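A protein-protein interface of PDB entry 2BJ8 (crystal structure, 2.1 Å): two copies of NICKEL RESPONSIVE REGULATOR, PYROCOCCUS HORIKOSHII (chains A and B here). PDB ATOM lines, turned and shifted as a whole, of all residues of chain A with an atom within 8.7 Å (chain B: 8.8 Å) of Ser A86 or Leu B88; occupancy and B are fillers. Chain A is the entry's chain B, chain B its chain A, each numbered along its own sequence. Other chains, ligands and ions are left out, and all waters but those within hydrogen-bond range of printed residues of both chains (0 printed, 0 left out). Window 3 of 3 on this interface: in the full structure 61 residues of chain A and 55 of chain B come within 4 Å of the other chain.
Of the 19 printed residues of chain B, 5 touch a printed residue of chain A.
Among the printed residues, 9 pairs touch across the chains.
Among the printed residues, no Asp or Glu carboxylate lies within 4 Å of a Lys or Arg side-chain nitrogen of the other chain.
OG1 of Thr A57 lies within hydrogen-bond range of OG1 of Thr B59, 2.8 Å away.
Of the printed residues of chain B, Ser A86 touches Leu B88 (3.6 Å).
Leu B88 touches just these residues of chain A: Ser A86 (3.6 Å) and Val A102 (3.5 Å).
No residue of chain A comes within 4 Å of Ser B87.
Of the printed residues of chain A, Val B100 touches Thr A57, Val A100 and Val A102.
Printed residues of chain B within 4 Å of Val A100: Val B100.
Of the printed residues of chain B, Ile A85 touches Val B90.
Of the printed residues of chain B, Thr A57 touches Thr B59 (2.8 Å) and Val B100 (3.4 Å).
Of the printed residues of chain A, Val B90 touches Ile A85 (3.6 Å) and Val A102 (3.9 Å).
Ile B60 touches none of the printed residues of chain A.
Ile B58 touches none of the printed residues of chain A.
The nearest residue of chain B that does not touch Ser A86 is Val B90 (4.5 Å).
The nearest printed residue of chain A that does not touch Val B100 is Leu A88 (4.4 Å).
Ser A86 touches Leu B88, but with the chains exchanged Leu A88 does not touch Ser B86 (4.3 Å).
Leu A88 touches Val B102, and with the chains exchanged Val A102 touches Leu B88.
Val B100 touches its own counterpart, Val A100.
Val A102 touches Val B100, but with the chains exchanged Val A100 does not touch Val B102 (4.2 Å).
Positions printed for both chains: 58, 77, 84, 85, 86, 87, 88, 89, 99, 100, 101 and 102.
Thr A57 touches Val B100.
CG1 of Val B90 touches CD1 of Ile A85, 3.6 Å away.
Leu B88 touches Ser A86 (CD2 to OG, 3.6 Å).
Val B102 touches Leu A88 (CG2 to CD2, 3.4 Å).
CG2 of Val A100 touches CG1 of Val B100, at 3.5 Å.
Leu B88 touches Val A102 (CD2 to CG2, 3.5 Å).
Val B90 touches Val A102.
Val A102 touches Val B100 (CG2 to CG2, 3.9 Å).
N of Val B102 lies within hydrogen-bond range of O of Ser B86, 2.9 Å away.
The backbone NH of Leu B88 is in hydrogen-bond range of the backbone carbonyl oxygen of Val B100 (2.8 Å).
N of Val B90 sits at hydrogen-bond distance from O of Leu B98 (2.9 Å).
The backbone NH (N) of Ile A85 is in hydrogen-bond range of the backbone carbonyl oxygen (O) of Val A102 (3.0 Å).
The backbone carbonyl oxygen (O) of Ser A86 lies within hydrogen-bond range of the backbone NH (N) of Val A102.
N of Val A100 lies within hydrogen-bond range of O of Leu A88.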
ATOM      1  N   GLY A  56      18.952 -11.992  14.014  1.00  0.00           N
ATOM      2  CA  GLY A  56      18.841 -12.733  12.778  1.00  0.00           C
ATOM      3  C   GLY A  56      20.117 -12.775  11.975  1.00  0.00           C
ATOM      4  O   GLY A  56      21.136 -12.191  12.350  1.00  0.00           O
ATOM      5  N   THR A  57      20.063 -13.498  10.867  1.00  0.00           N
ATOM      6  CA  THR A  57      21.206 -13.604   9.982  1.00  0.00           C
ATOM      7  C   THR A  57      20.725 -13.392   8.558  1.00  0.00           C
ATOM      8  O   THR A  57      19.595 -13.730   8.215  1.00  0.00           O
ATOM      9  CB  THR A  57      21.904 -14.991  10.087  1.00  0.00           C
ATOM     10  OG1 THR A  57      20.968 -16.032   9.785  1.00  0.00           O
ATOM     11  CG2 THR A  57      22.455 -15.203  11.488  1.00  0.00           C
ATOM     12  N   ILE A  58      21.584 -12.801   7.742  1.00  0.00           N
ATOM     13  CA  ILE A  58      21.269 -12.557   6.347  1.00  0.00           C
ATOM     14  C   ILE A  58      22.377 -13.209   5.531  1.00  0.00           C
ATOM     15  O   ILE A  58      23.534 -12.793   5.597  1.00  0.00           O
ATOM     16  CB  ILE A  58      21.207 -11.043   6.033  1.00  0.00           C
ATOM     17  CG1 ILE A  58      20.175 -10.365   6.947  1.00  0.00           C
ATOM     18  CG2 ILE A  58      20.812 -10.831   4.567  1.00  0.00           C
ATOM     19  CD1 ILE A  58      20.130  -8.852   6.829  1.00  0.00           C
ATOM     20  N   GLN A  77      25.764  -1.642   4.685  1.00  0.00           N
ATOM     21  CA  GLN A  77      26.055  -2.153   6.018  1.00  0.00           C
ATOM     22  C   GLN A  77      26.613  -1.121   6.986  1.00  0.00           C
ATOM     23  O   GLN A  77      26.227  -1.096   8.156  1.00  0.00           O
ATOM     24  CB  GLN A  77      27.005  -3.348   5.930  1.00  0.00           C
ATOM     25  CG  GLN A  77      26.374  -4.569   5.277  1.00  0.00           C
ATOM     26  CD  GLN A  77      27.298  -5.767   5.269  1.00  0.00           C
ATOM     27  OE1 GLN A  77      27.671  -6.290   6.323  1.00  0.00           O
ATOM     28  NE2 GLN A  77      27.674  -6.211   4.075  1.00  0.00           N
ATOM     29  N   TYR A  80      24.214   0.893   8.954  1.00  0.00           N
ATOM     30  CA  TYR A  80      23.496   0.273  10.065  1.00  0.00           C
ATOM     31  C   TYR A  80      24.429  -0.326  11.108  1.00  0.00           C
ATOM     32  O   TYR A  80      24.240  -1.462  11.532  1.00  0.00           O
ATOM     33  CB  TYR A  80      22.558  -0.827   9.547  1.00  0.00           C
ATOM     34  CG  TYR A  80      21.439  -0.330   8.652  1.00  0.00           C
ATOM     35  CD1 TYR A  80      21.608  -0.238   7.271  1.00  0.00           C
ATOM     36  CD2 TYR A  80      20.217   0.066   9.193  1.00  0.00           C
ATOM     37  CE1 TYR A  80      20.584   0.235   6.446  1.00  0.00           C
ATOM     38  CE2 TYR A  80      19.188   0.543   8.383  1.00  0.00           C
ATOM     39  CZ  TYR A  80      19.378   0.624   7.014  1.00  0.00           C
ATOM     40  OH  TYR A  80      18.356   1.093   6.219  1.00  0.00           O
ATOM     41  N   LEU A  81      25.420   0.450  11.531  1.00  0.00           N
ATOM     42  CA  LEU A  81      26.402  -0.001  12.513  1.00  0.00           C
ATOM     43  C   LEU A  81      25.791  -0.485  13.814  1.00  0.00           C
ATOM     44  O   LEU A  81      26.368  -1.324  14.497  1.00  0.00           O
ATOM     45  CB  LEU A  81      27.390   1.125  12.825  1.00  0.00           C
ATOM     46  CG  LEU A  81      28.128   1.692  11.621  1.00  0.00           C
ATOM     47  CD1 LEU A  81      29.008   2.844  12.051  1.00  0.00           C
ATOM     48  CD2 LEU A  81      28.949   0.588  10.979  1.00  0.00           C
ATOM     49  N   GLU A  83      22.830  -2.124  14.208  1.00  0.00           N
ATOM     50  CA  GLU A  83      22.144  -3.413  14.109  1.00  0.00           C
ATOM     51  C   GLU A  83      23.056  -4.551  13.669  1.00  0.00           C
ATOM     52  O   GLU A  83      22.904  -5.687  14.119  1.00  0.00           O
ATOM     53  CB  GLU A  83      20.952  -3.327  13.150  1.00  0.00           C
ATOM     54  CG  GLU A  83      19.790  -2.504  13.683  1.00  0.00           C
ATOM     55  CD  GLU A  83      20.029  -1.009  13.591  1.00  0.00           C
ATOM     56  OE1 GLU A  83      19.349  -0.260  14.322  1.00  0.00           O
ATOM     57  OE2 GLU A  83      20.883  -0.582  12.783  1.00  0.00           O
ATOM     58  N   ILE A  84      23.996  -4.254  12.782  1.00  0.00           N
ATOM     59  CA  ILE A  84      24.910  -5.283  12.309  1.00  0.00           C
ATOM     60  C   ILE A  84      26.069  -5.493  13.278  1.00  0.00           C
ATOM     61  O   ILE A  84      26.820  -4.569  13.586  1.00  0.00           O
ATOM     62  CB  ILE A  84      25.457  -4.934  10.930  1.00  0.00           C
ATOM     63  CG1 ILE A  84      24.295  -4.892   9.932  1.00  0.00           C
ATOM     64  CG2 ILE A  84      26.524  -5.954  10.525  1.00  0.00           C
ATOM     65  CD1 ILE A  84      24.683  -4.425   8.541  1.00  0.00           C
ATOM     66  N   ILE A  85      26.207  -6.724  13.756  1.00  0.00           N
ATOM     67  CA  ILE A  85      27.256  -7.065  14.706  1.00  0.00           C
ATOM     68  C   ILE A  85      28.563  -7.413  14.006  1.00  0.00           C
ATOM     69  O   ILE A  85      29.610  -6.866  14.330  1.00  0.00           O
ATOM     70  CB  ILE A  85      26.819  -8.250  15.581  1.00  0.00           C
ATOM     71  CG1 ILE A  85      25.537  -7.881  16.328  1.00  0.00           C
ATOM     72  CG2 ILE A  85      27.917  -8.613  16.571  1.00  0.00           C
ATOM     73  CD1 ILE A  85      24.997  -8.997  17.186  1.00  0.00           C
ATOM     74  N   SER A  86      28.491  -8.330  13.049  1.00  0.00           N
ATOM     75  CA  SER A  86      29.665  -8.756  12.302  1.00  0.00           C
ATOM     76  C   SER A  86      29.203  -9.624  11.151  1.00  0.00           C
ATOM     77  O   SER A  86      28.012  -9.932  11.037  1.00  0.00           O
ATOM     78  CB  SER A  86      30.611  -9.563  13.201  1.00  0.00           C
ATOM     79  OG  SER A  86      29.980 -10.754  13.629  1.00  0.00           O
ATOM     80  N   SER A  87      30.141 -10.015  10.295  1.00  0.00           N
ATOM     81  CA  SER A  87      29.811 -10.855   9.154  1.00  0.00           C
ATOM     82  C   SER A  87      30.922 -11.846   8.848  1.00  0.00           C
ATOM     83  O   SER A  87      32.106 -11.575   9.088  1.00  0.00           O
ATOM     84  CB  SER A  87      29.537  -9.993   7.924  1.00  0.00           C
ATOM     85  OG  SER A  87      30.649  -9.182   7.625  1.00  0.00           O
ATOM     86  N   LEU A  88      30.524 -13.000   8.327  1.00  0.00           N
ATOM     87  CA  LEU A  88      31.461 -14.051   7.972  1.00  0.00           C
ATOM     88  C   LEU A  88      31.463 -14.179   6.452  1.00  0.00           C
ATOM     89  O   LEU A  88      30.403 -14.257   5.818  1.00  0.00           O
ATOM     90  CB  LEU A  88      31.037 -15.363   8.631  1.00  0.00           C
ATOM     91  CG  LEU A  88      31.910 -16.599   8.415  1.00  0.00           C
ATOM     92  CD1 LEU A  88      33.347 -16.292   8.788  1.00  0.00           C
ATOM     93  CD2 LEU A  88      31.367 -17.736   9.268  1.00  0.00           C
ATOM     94  N   HIS A  89      32.657 -14.181   5.869  1.00  0.00           N
ATOM     95  CA  HIS A  89      32.793 -14.275   4.424  1.00  0.00           C
ATOM     96  C   HIS A  89      33.595 -15.504   4.030  1.00  0.00           C
ATOM     97  O   HIS A  89      34.619 -15.811   4.637  1.00  0.00           O
ATOM     98  CB  HIS A  89      33.467 -13.004   3.890  1.00  0.00           C
ATOM     99  CG  HIS A  89      33.645 -12.980   2.404  1.00  0.00           C
ATOM    100  ND1 HIS A  89      33.254 -11.908   1.630  1.00  0.00           N
ATOM    101  CD2 HIS A  89      34.216 -13.868   1.556  1.00  0.00           C
ATOM    102  CE1 HIS A  89      33.583 -12.134   0.371  1.00  0.00           C
ATOM    103  NE2 HIS A  89      34.168 -13.317   0.300  1.00  0.00           N
ATOM    104  N   GLU A  99      28.448 -14.695   1.998  1.00  0.00           N
ATOM    105  CA  GLU A  99      28.583 -13.861   3.176  1.00  0.00           C
ATOM    106  C   GLU A  99      27.362 -13.978   4.071  1.00  0.00           C
ATOM    107  O   GLU A  99      26.228 -13.969   3.585  1.00  0.00           O
ATOM    108  CB  GLU A  99      28.772 -12.406   2.746  1.00  0.00           C
ATOM    109  CG  GLU A  99      29.172 -11.456   3.857  1.00  0.00           C
ATOM    110  CD  GLU A  99      29.345 -10.031   3.361  1.00  0.00           C
ATOM    111  OE1 GLU A  99      29.894  -9.848   2.251  1.00  0.00           O
ATOM    112  OE2 GLU A  99      28.940  -9.093   4.083  1.00  0.00           O
ATOM    113  N   VAL A 100      27.583 -14.113   5.374  1.00  0.00           N
ATOM    114  CA  VAL A 100      26.466 -14.182   6.301  1.00  0.00           C
ATOM    115  C   VAL A 100      26.625 -13.054   7.322  1.00  0.00           C
ATOM    116  O   VAL A 100      27.657 -12.930   7.982  1.00  0.00           O
ATOM    117  CB  VAL A 100      26.366 -15.570   6.997  1.00  0.00           C
ATOM    118  CG1 VAL A 100      27.689 -15.952   7.628  1.00  0.00           C
ATOM    119  CG2 VAL A 100      25.254 -15.544   8.041  1.00  0.00           C
ATOM    120  N   ILE A 101      25.587 -12.229   7.430  1.00  0.00           N
ATOM    121  CA  ILE A 101      25.581 -11.075   8.324  1.00  0.00           C
ATOM    122  C   ILE A 101      24.710 -11.299   9.560  1.00  0.00           C
ATOM    123  O   ILE A 101      23.534 -11.643   9.440  1.00  0.00           O
ATOM    124  CB  ILE A 101      25.065  -9.834   7.557  1.00  0.00           C
ATOM    125  CG1 ILE A 101      25.857  -9.677   6.257  1.00  0.00           C
ATOM    126  CG2 ILE A 101      25.182  -8.586   8.414  1.00  0.00           C
ATOM    127  CD1 ILE A 101      25.271  -8.691   5.288  1.00  0.00           C
ATOM    128  N   VAL A 102      25.287 -11.116  10.745  1.00  0.00           N
ATOM    129  CA  VAL A 102      24.536 -11.287  11.983  1.00  0.00           C
ATOM    130  C   VAL A 102      23.996  -9.917  12.384  1.00  0.00           C
ATOM    131  O   VAL A 102      24.738  -8.934  12.451  1.00  0.00           O
ATOM    132  CB  VAL A 102      25.419 -11.861  13.126  1.00  0.00           C
ATOM    133  CG1 VAL A 102      24.609 -11.973  14.414  1.00  0.00           C
ATOM    134  CG2 VAL A 102      25.937 -13.236  12.743  1.00  0.00           C
ATOM    135  N   VAL A 103      22.695  -9.860  12.640  1.00  0.00           N
ATOM    136  CA  VAL A 103      22.039  -8.614  13.010  1.00  0.00           C
ATOM    137  C   VAL A 103      21.258  -8.764  14.302  1.00  0.00           C
ATOM    138  O   VAL A 103      20.757  -9.841  14.616  1.00  0.00           O
ATOM    139  CB  VAL A 103      21.073  -8.145  11.899  1.00  0.00           C
ATOM    140  CG1 VAL A 103      21.833  -7.945  10.606  1.00  0.00           C
ATOM    141  CG2 VAL A 103      19.969  -9.176  11.694  1.00  0.00           C
ATOM    142  N   LYS A 104      21.156  -7.668  15.044  1.00  0.00           N
ATOM    143  CA  LYS A 104      20.440  -7.658  16.308  1.00  0.00           C
ATOM    144  C   LYS A 104      19.822  -6.275  16.444  1.00  0.00           C
ATOM    145  O   LYS A 104      20.493  -5.272  16.230  1.00  0.00           O
ATOM    146  CB  LYS A 104      21.413  -7.932  17.457  1.00  0.00           C
ATOM    147  CG  LYS A 104      20.762  -8.135  18.806  1.00  0.00           C
ATOM    148  CD  LYS A 104      21.804  -8.422  19.881  1.00  0.00           C
ATOM    149  CE  LYS A 104      21.145  -8.714  21.222  1.00  0.00           C
ATOM    150  NZ  LYS A 104      22.140  -8.902  22.318  1.00  0.00           N
ATOM    151  N   ILE B  58      23.852 -22.400   8.784  1.00  0.00           N
ATOM    152  CA  ILE B  58      22.956 -22.955   9.767  1.00  0.00           C
ATOM    153  C   ILE B  58      23.015 -21.991  10.941  1.00  0.00           C
ATOM    154  O   ILE B  58      24.068 -21.818  11.556  1.00  0.00           O
ATOM    155  CB  ILE B  58      23.413 -24.360  10.210  1.00  0.00           C
ATOM    156  CG1 ILE B  58      23.494 -25.290   8.996  1.00  0.00           C
ATOM    157  CG2 ILE B  58      22.441 -24.918  11.238  1.00  0.00           C
ATOM    158  CD1 ILE B  58      24.098 -26.643   9.304  1.00  0.00           C
ATOM    159  N   THR B  59      21.892 -21.344  11.228  1.00  0.00           N
ATOM    160  CA  THR B  59      21.818 -20.395  12.334  1.00  0.00           C
ATOM    161  C   THR B  59      21.167 -21.061  13.537  1.00  0.00           C
ATOM    162  O   THR B  59      20.119 -21.693  13.414  1.00  0.00           O
ATOM    163  CB  THR B  59      20.984 -19.165  11.948  1.00  0.00           C
ATOM    164  OG1 THR B  59      21.538 -18.557  10.774  1.00  0.00           O
ATOM    165  CG2 THR B  59      20.979 -18.152  13.075  1.00  0.00           C
ATOM    166  N   ILE B  60      21.788 -20.933  14.703  1.00  0.00           N
ATOM    167  CA  ILE B  60      21.223 -21.534  15.893  1.00  0.00           C
ATOM    168  C   ILE B  60      21.401 -20.637  17.097  1.00  0.00           C
ATOM    169  O   ILE B  60      22.322 -19.819  17.151  1.00  0.00           O
ATOM    170  CB  ILE B  60      21.853 -22.923  16.211  1.00  0.00           C
ATOM    171  CG1 ILE B  60      23.336 -22.776  16.528  1.00  0.00           C
ATOM    172  CG2 ILE B  60      21.669 -23.870  15.026  1.00  0.00           C
ATOM    173  CD1 ILE B  60      23.973 -24.050  17.039  1.00  0.00           C
ATOM    174  N   TYR B  62      21.130 -20.782  21.505  1.00  0.00           N
ATOM    175  CA  TYR B  62      21.056 -21.657  22.663  1.00  0.00           C
ATOM    176  C   TYR B  62      21.664 -21.029  23.901  1.00  0.00           C
ATOM    177  O   TYR B  62      22.367 -20.015  23.833  1.00  0.00           O
ATOM    178  CB  TYR B  62      21.775 -22.977  22.369  1.00  0.00           C
ATOM    179  CG  TYR B  62      23.219 -22.795  21.957  1.00  0.00           C
ATOM    180  CD1 TYR B  62      24.237 -22.700  22.908  1.00  0.00           C
ATOM    181  CD2 TYR B  62      23.563 -22.675  20.611  1.00  0.00           C
ATOM    182  CE1 TYR B  62      25.564 -22.487  22.523  1.00  0.00           C
ATOM    183  CE2 TYR B  62      24.883 -22.457  20.215  1.00  0.00           C
ATOM    184  CZ  TYR B  62      25.876 -22.364  21.174  1.00  0.00           C
ATOM    185  OH  TYR B  62      27.174 -22.136  20.775  1.00  0.00           O
ATOM    186  N   GLN B  77      29.931 -31.222  15.036  1.00  0.00           N
ATOM    187  CA  GLN B  77      30.593 -30.444  13.995  1.00  0.00           C
ATOM    188  C   GLN B  77      31.949 -31.020  13.623  1.00  0.00           C
ATOM    189  O   GLN B  77      32.319 -31.050  12.449  1.00  0.00           O
ATOM    190  CB  GLN B  77      30.755 -28.982  14.431  1.00  0.00           C
ATOM    191  CG  GLN B  77      29.447 -28.203  14.449  1.00  0.00           C
ATOM    192  CD  GLN B  77      29.630 -26.741  14.818  1.00  0.00           C
ATOM    193  OE1 GLN B  77      30.320 -25.991  14.128  1.00  0.00           O
ATOM    194  NE2 GLN B  77      29.010 -26.332  15.913  1.00  0.00           N
ATOM    195  N   ILE B  84      31.799 -28.604   7.078  1.00  0.00           N
ATOM    196  CA  ILE B  84      31.772 -27.384   7.877  1.00  0.00           C
ATOM    197  C   ILE B  84      33.035 -26.547   7.675  1.00  0.00           C
ATOM    198  O   ILE B  84      34.132 -26.963   8.033  1.00  0.00           O
ATOM    199  CB  ILE B  84      31.596 -27.715   9.371  1.00  0.00           C
ATOM    200  CG1 ILE B  84      30.240 -28.394   9.582  1.00  0.00           C
ATOM    201  CG2 ILE B  84      31.689 -26.443  10.208  1.00  0.00           C
ATOM    202  CD1 ILE B  84      29.973 -28.800  11.012  1.00  0.00           C
ATOM    203  N   ILE B  85      32.856 -25.365   7.092  1.00  0.00           N
ATOM    204  CA  ILE B  85      33.950 -24.444   6.808  1.00  0.00           C
ATOM    205  C   ILE B  85      34.425 -23.662   8.030  1.00  0.00           C
ATOM    206  O   ILE B  85      35.608 -23.687   8.363  1.00  0.00           O
ATOM    207  CB  ILE B  85      33.535 -23.427   5.724  1.00  0.00           C
ATOM    208  CG1 ILE B  85      33.148 -24.163   4.442  1.00  0.00           C
ATOM    209  CG2 ILE B  85      34.673 -22.456   5.452  1.00  0.00           C
ATOM    210  CD1 ILE B  85      32.606 -23.257   3.360  1.00  0.00           C
ATOM    211  N   SER B  86      33.491 -22.968   8.681  1.00  0.00           N
ATOM    212  CA  SER B  86      33.767 -22.143   9.856  1.00  0.00           C
ATOM    213  C   SER B  86      32.443 -21.784  10.515  1.00  0.00           C
ATOM    214  O   SER B  86      31.379 -22.018   9.952  1.00  0.00           O
ATOM    215  CB  SER B  86      34.447 -20.830   9.452  1.00  0.00           C
ATOM    216  OG  SER B  86      35.684 -21.049   8.804  1.00  0.00           O
ATOM    217  N   SER B  87      32.513 -21.205  11.708  1.00  0.00           N
ATOM    218  CA  SER B  87      31.307 -20.779  12.407  1.00  0.00           C
ATOM    219  C   SER B  87      31.552 -19.445  13.100  1.00  0.00           C
ATOM    220  O   SER B  87      32.651 -19.169  13.588  1.00  0.00           O
ATOM    221  CB  SER B  87      30.863 -21.824  13.433  1.00  0.00           C
ATOM    222  OG  SER B  87      31.801 -21.948  14.479  1.00  0.00           O
ATOM    223  N   LEU B  88      30.517 -18.613  13.117  1.00  0.00           N
ATOM    224  CA  LEU B  88      30.577 -17.305  13.748  1.00  0.00           C
ATOM    225  C   LEU B  88      29.750 -17.387  15.026  1.00  0.00           C
ATOM    226  O   LEU B  88      28.671 -17.972  15.036  1.00  0.00           O
ATOM    227  CB  LEU B  88      30.004 -16.250  12.806  1.00  0.00           C
ATOM    228  CG  LEU B  88      29.928 -14.797  13.280  1.00  0.00           C
ATOM    229  CD1 LEU B  88      31.310 -14.289  13.645  1.00  0.00           C
ATOM    230  CD2 LEU B  88      29.329 -13.952  12.167  1.00  0.00           C
ATOM    231  N   HIS B  89      30.264 -16.814  16.108  1.00  0.00           N
ATOM    232  CA  HIS B  89      29.559 -16.857  17.380  1.00  0.00           C
ATOM    233  C   HIS B  89      29.411 -15.457  17.973  1.00  0.00           C
ATOM    234  O   HIS B  89      30.358 -14.677  17.982  1.00  0.00           O
ATOM    235  CB  HIS B  89      30.317 -17.773  18.344  1.00  0.00           C
ATOM    236  CG  HIS B  89      29.646 -17.972  19.668  1.00  0.00           C
ATOM    237  ND1 HIS B  89      29.380 -19.225  20.182  1.00  0.00           N
ATOM    238  CD2 HIS B  89      29.273 -17.089  20.626  1.00  0.00           C
ATOM    239  CE1 HIS B  89      28.882 -19.104  21.399  1.00  0.00           C
ATOM    240  NE2 HIS B  89      28.808 -17.818  21.694  1.00  0.00           N
ATOM    241  N   VAL B  90      28.204 -15.147  18.439  1.00  0.00           N
ATOM    242  CA  VAL B  90      27.917 -13.864  19.069  1.00  0.00           C
ATOM    243  C   VAL B  90      27.289 -14.123  20.446  1.00  0.00           C
ATOM    244  O   VAL B  90      26.250 -14.776  20.543  1.00  0.00           O
ATOM    245  CB  VAL B  90      26.928 -13.019  18.228  1.00  0.00           C
ATOM    246  CG1 VAL B  90      26.614 -11.714  18.950  1.00  0.00           C
ATOM    247  CG2 VAL B  90      27.518 -12.722  16.858  1.00  0.00           C
ATOM    248  N   HIS B  91      27.933 -13.631  21.502  1.00  0.00           N
ATOM    249  CA  HIS B  91      27.423 -13.791  22.867  1.00  0.00           C
ATOM    250  C   HIS B  91      26.350 -12.725  23.059  1.00  0.00           C
ATOM    251  O   HIS B  91      26.657 -11.531  23.154  1.00  0.00           O
ATOM    252  CB  HIS B  91      28.542 -13.589  23.883  1.00  0.00           C
ATOM    253  CG  HIS B  91      29.788 -14.350  23.559  1.00  0.00           C
ATOM    254  ND1 HIS B  91      29.801 -15.716  23.376  1.00  0.00           N
ATOM    255  CD2 HIS B  91      31.069 -13.936  23.401  1.00  0.00           C
ATOM    256  CE1 HIS B  91      31.037 -16.112  23.124  1.00  0.00           C
ATOM    257  NE2 HIS B  91      31.826 -15.051  23.133  1.00  0.00           N
ATOM    258  N   CYS B  97      23.686 -17.646  23.332  1.00  0.00           N
ATOM    259  CA  CYS B  97      24.632 -17.515  22.233  1.00  0.00           C
ATOM    260  C   CYS B  97      23.934 -17.721  20.899  1.00  0.00           C
ATOM    261  O   CYS B  97      23.005 -18.521  20.787  1.00  0.00           O
ATOM    262  CB  CYS B  97      25.740 -18.569  22.335  1.00  0.00           C
ATOM    263  SG  CYS B  97      26.716 -18.574  23.852  1.00  0.00           S
ATOM    264  N   LEU B  98      24.385 -16.989  19.889  1.00  0.00           N
ATOM    265  CA  LEU B  98      23.857 -17.151  18.552  1.00  0.00           C
ATOM    266  C   LEU B  98      25.066 -17.626  17.767  1.00  0.00           C
ATOM    267  O   LEU B  98      26.159 -17.073  17.908  1.00  0.00           O
ATOM    268  CB  LEU B  98      23.331 -15.835  17.981  1.00  0.00           C
ATOM    269  CG  LEU B  98      22.777 -16.007  16.560  1.00  0.00           C
ATOM    270  CD1 LEU B  98      21.677 -15.012  16.307  1.00  0.00           C
ATOM    271  CD2 LEU B  98      23.897 -15.856  15.546  1.00  0.00           C
ATOM    272  N   GLU B  99      24.879 -18.658  16.958  1.00  0.00           N
ATOM    273  CA  GLU B  99      25.976 -19.210  16.179  1.00  0.00           C
ATOM    274  C   GLU B  99      25.530 -19.428  14.738  1.00  0.00           C
ATOM    275  O   GLU B  99      24.382 -19.792  14.484  1.00  0.00           O
ATOM    276  CB  GLU B  99      26.418 -20.532  16.817  1.00  0.00           C
ATOM    277  CG  GLU B  99      27.685 -21.155  16.261  1.00  0.00           C
ATOM    278  CD  GLU B  99      28.045 -22.467  16.960  1.00  0.00           C
ATOM    279  OE1 GLU B  99      27.980 -22.521  18.209  1.00  0.00           O
ATOM    280  OE2 GLU B  99      28.406 -23.445  16.266  1.00  0.00           O
ATOM    281  N   VAL B 100      26.426 -19.169  13.792  1.00  0.00           N
ATOM    282  CA  VAL B 100      26.122 -19.377  12.384  1.00  0.00           C
ATOM    283  C   VAL B 100      27.217 -20.255  11.804  1.00  0.00           C
ATOM    284  O   VAL B 100      28.382 -19.871  11.779  1.00  0.00           O
ATOM    285  CB  VAL B 100      26.081 -18.064  11.576  1.00  0.00           C
ATOM    286  CG1 VAL B 100      25.526 -18.345  10.189  1.00  0.00           C
ATOM    287  CG2 VAL B 100      25.233 -17.039  12.275  1.00  0.00           C
ATOM    288  N   ILE B 101      26.828 -21.439  11.348  1.00  0.00           N
ATOM    289  CA  ILE B 101      27.752 -22.403  10.770  1.00  0.00           C
ATOM    290  C   ILE B 101      27.657 -22.384   9.247  1.00  0.00           C
ATOM    291  O   ILE B 101      26.576 -22.555   8.683  1.00  0.00           O
ATOM    292  CB  ILE B 101      27.421 -23.810  11.283  1.00  0.00           C
ATOM    293  CG1 ILE B 101      27.439 -23.804  12.813  1.00  0.00           C
ATOM    294  CG2 ILE B 101      28.406 -24.819  10.727  1.00  0.00           C
ATOM    295  CD1 ILE B 101      26.714 -24.962  13.447  1.00  0.00           C
ATOM    296  N   VAL B 102      28.785 -22.147   8.586  1.00  0.00           N
ATOM    297  CA  VAL B 102      28.826 -22.119   7.127  1.00  0.00           C
ATOM    298  C   VAL B 102      29.228 -23.504   6.623  1.00  0.00           C
ATOM    299  O   VAL B 102      30.215 -24.081   7.084  1.00  0.00           O
ATOM    300  CB  VAL B 102      29.842 -21.077   6.614  1.00  0.00           C
ATOM    301  CG1 VAL B 102      29.854 -21.061   5.102  1.00  0.00           C
ATOM    302  CG2 VAL B 102      29.486 -19.702   7.147  1.00  0.00           C
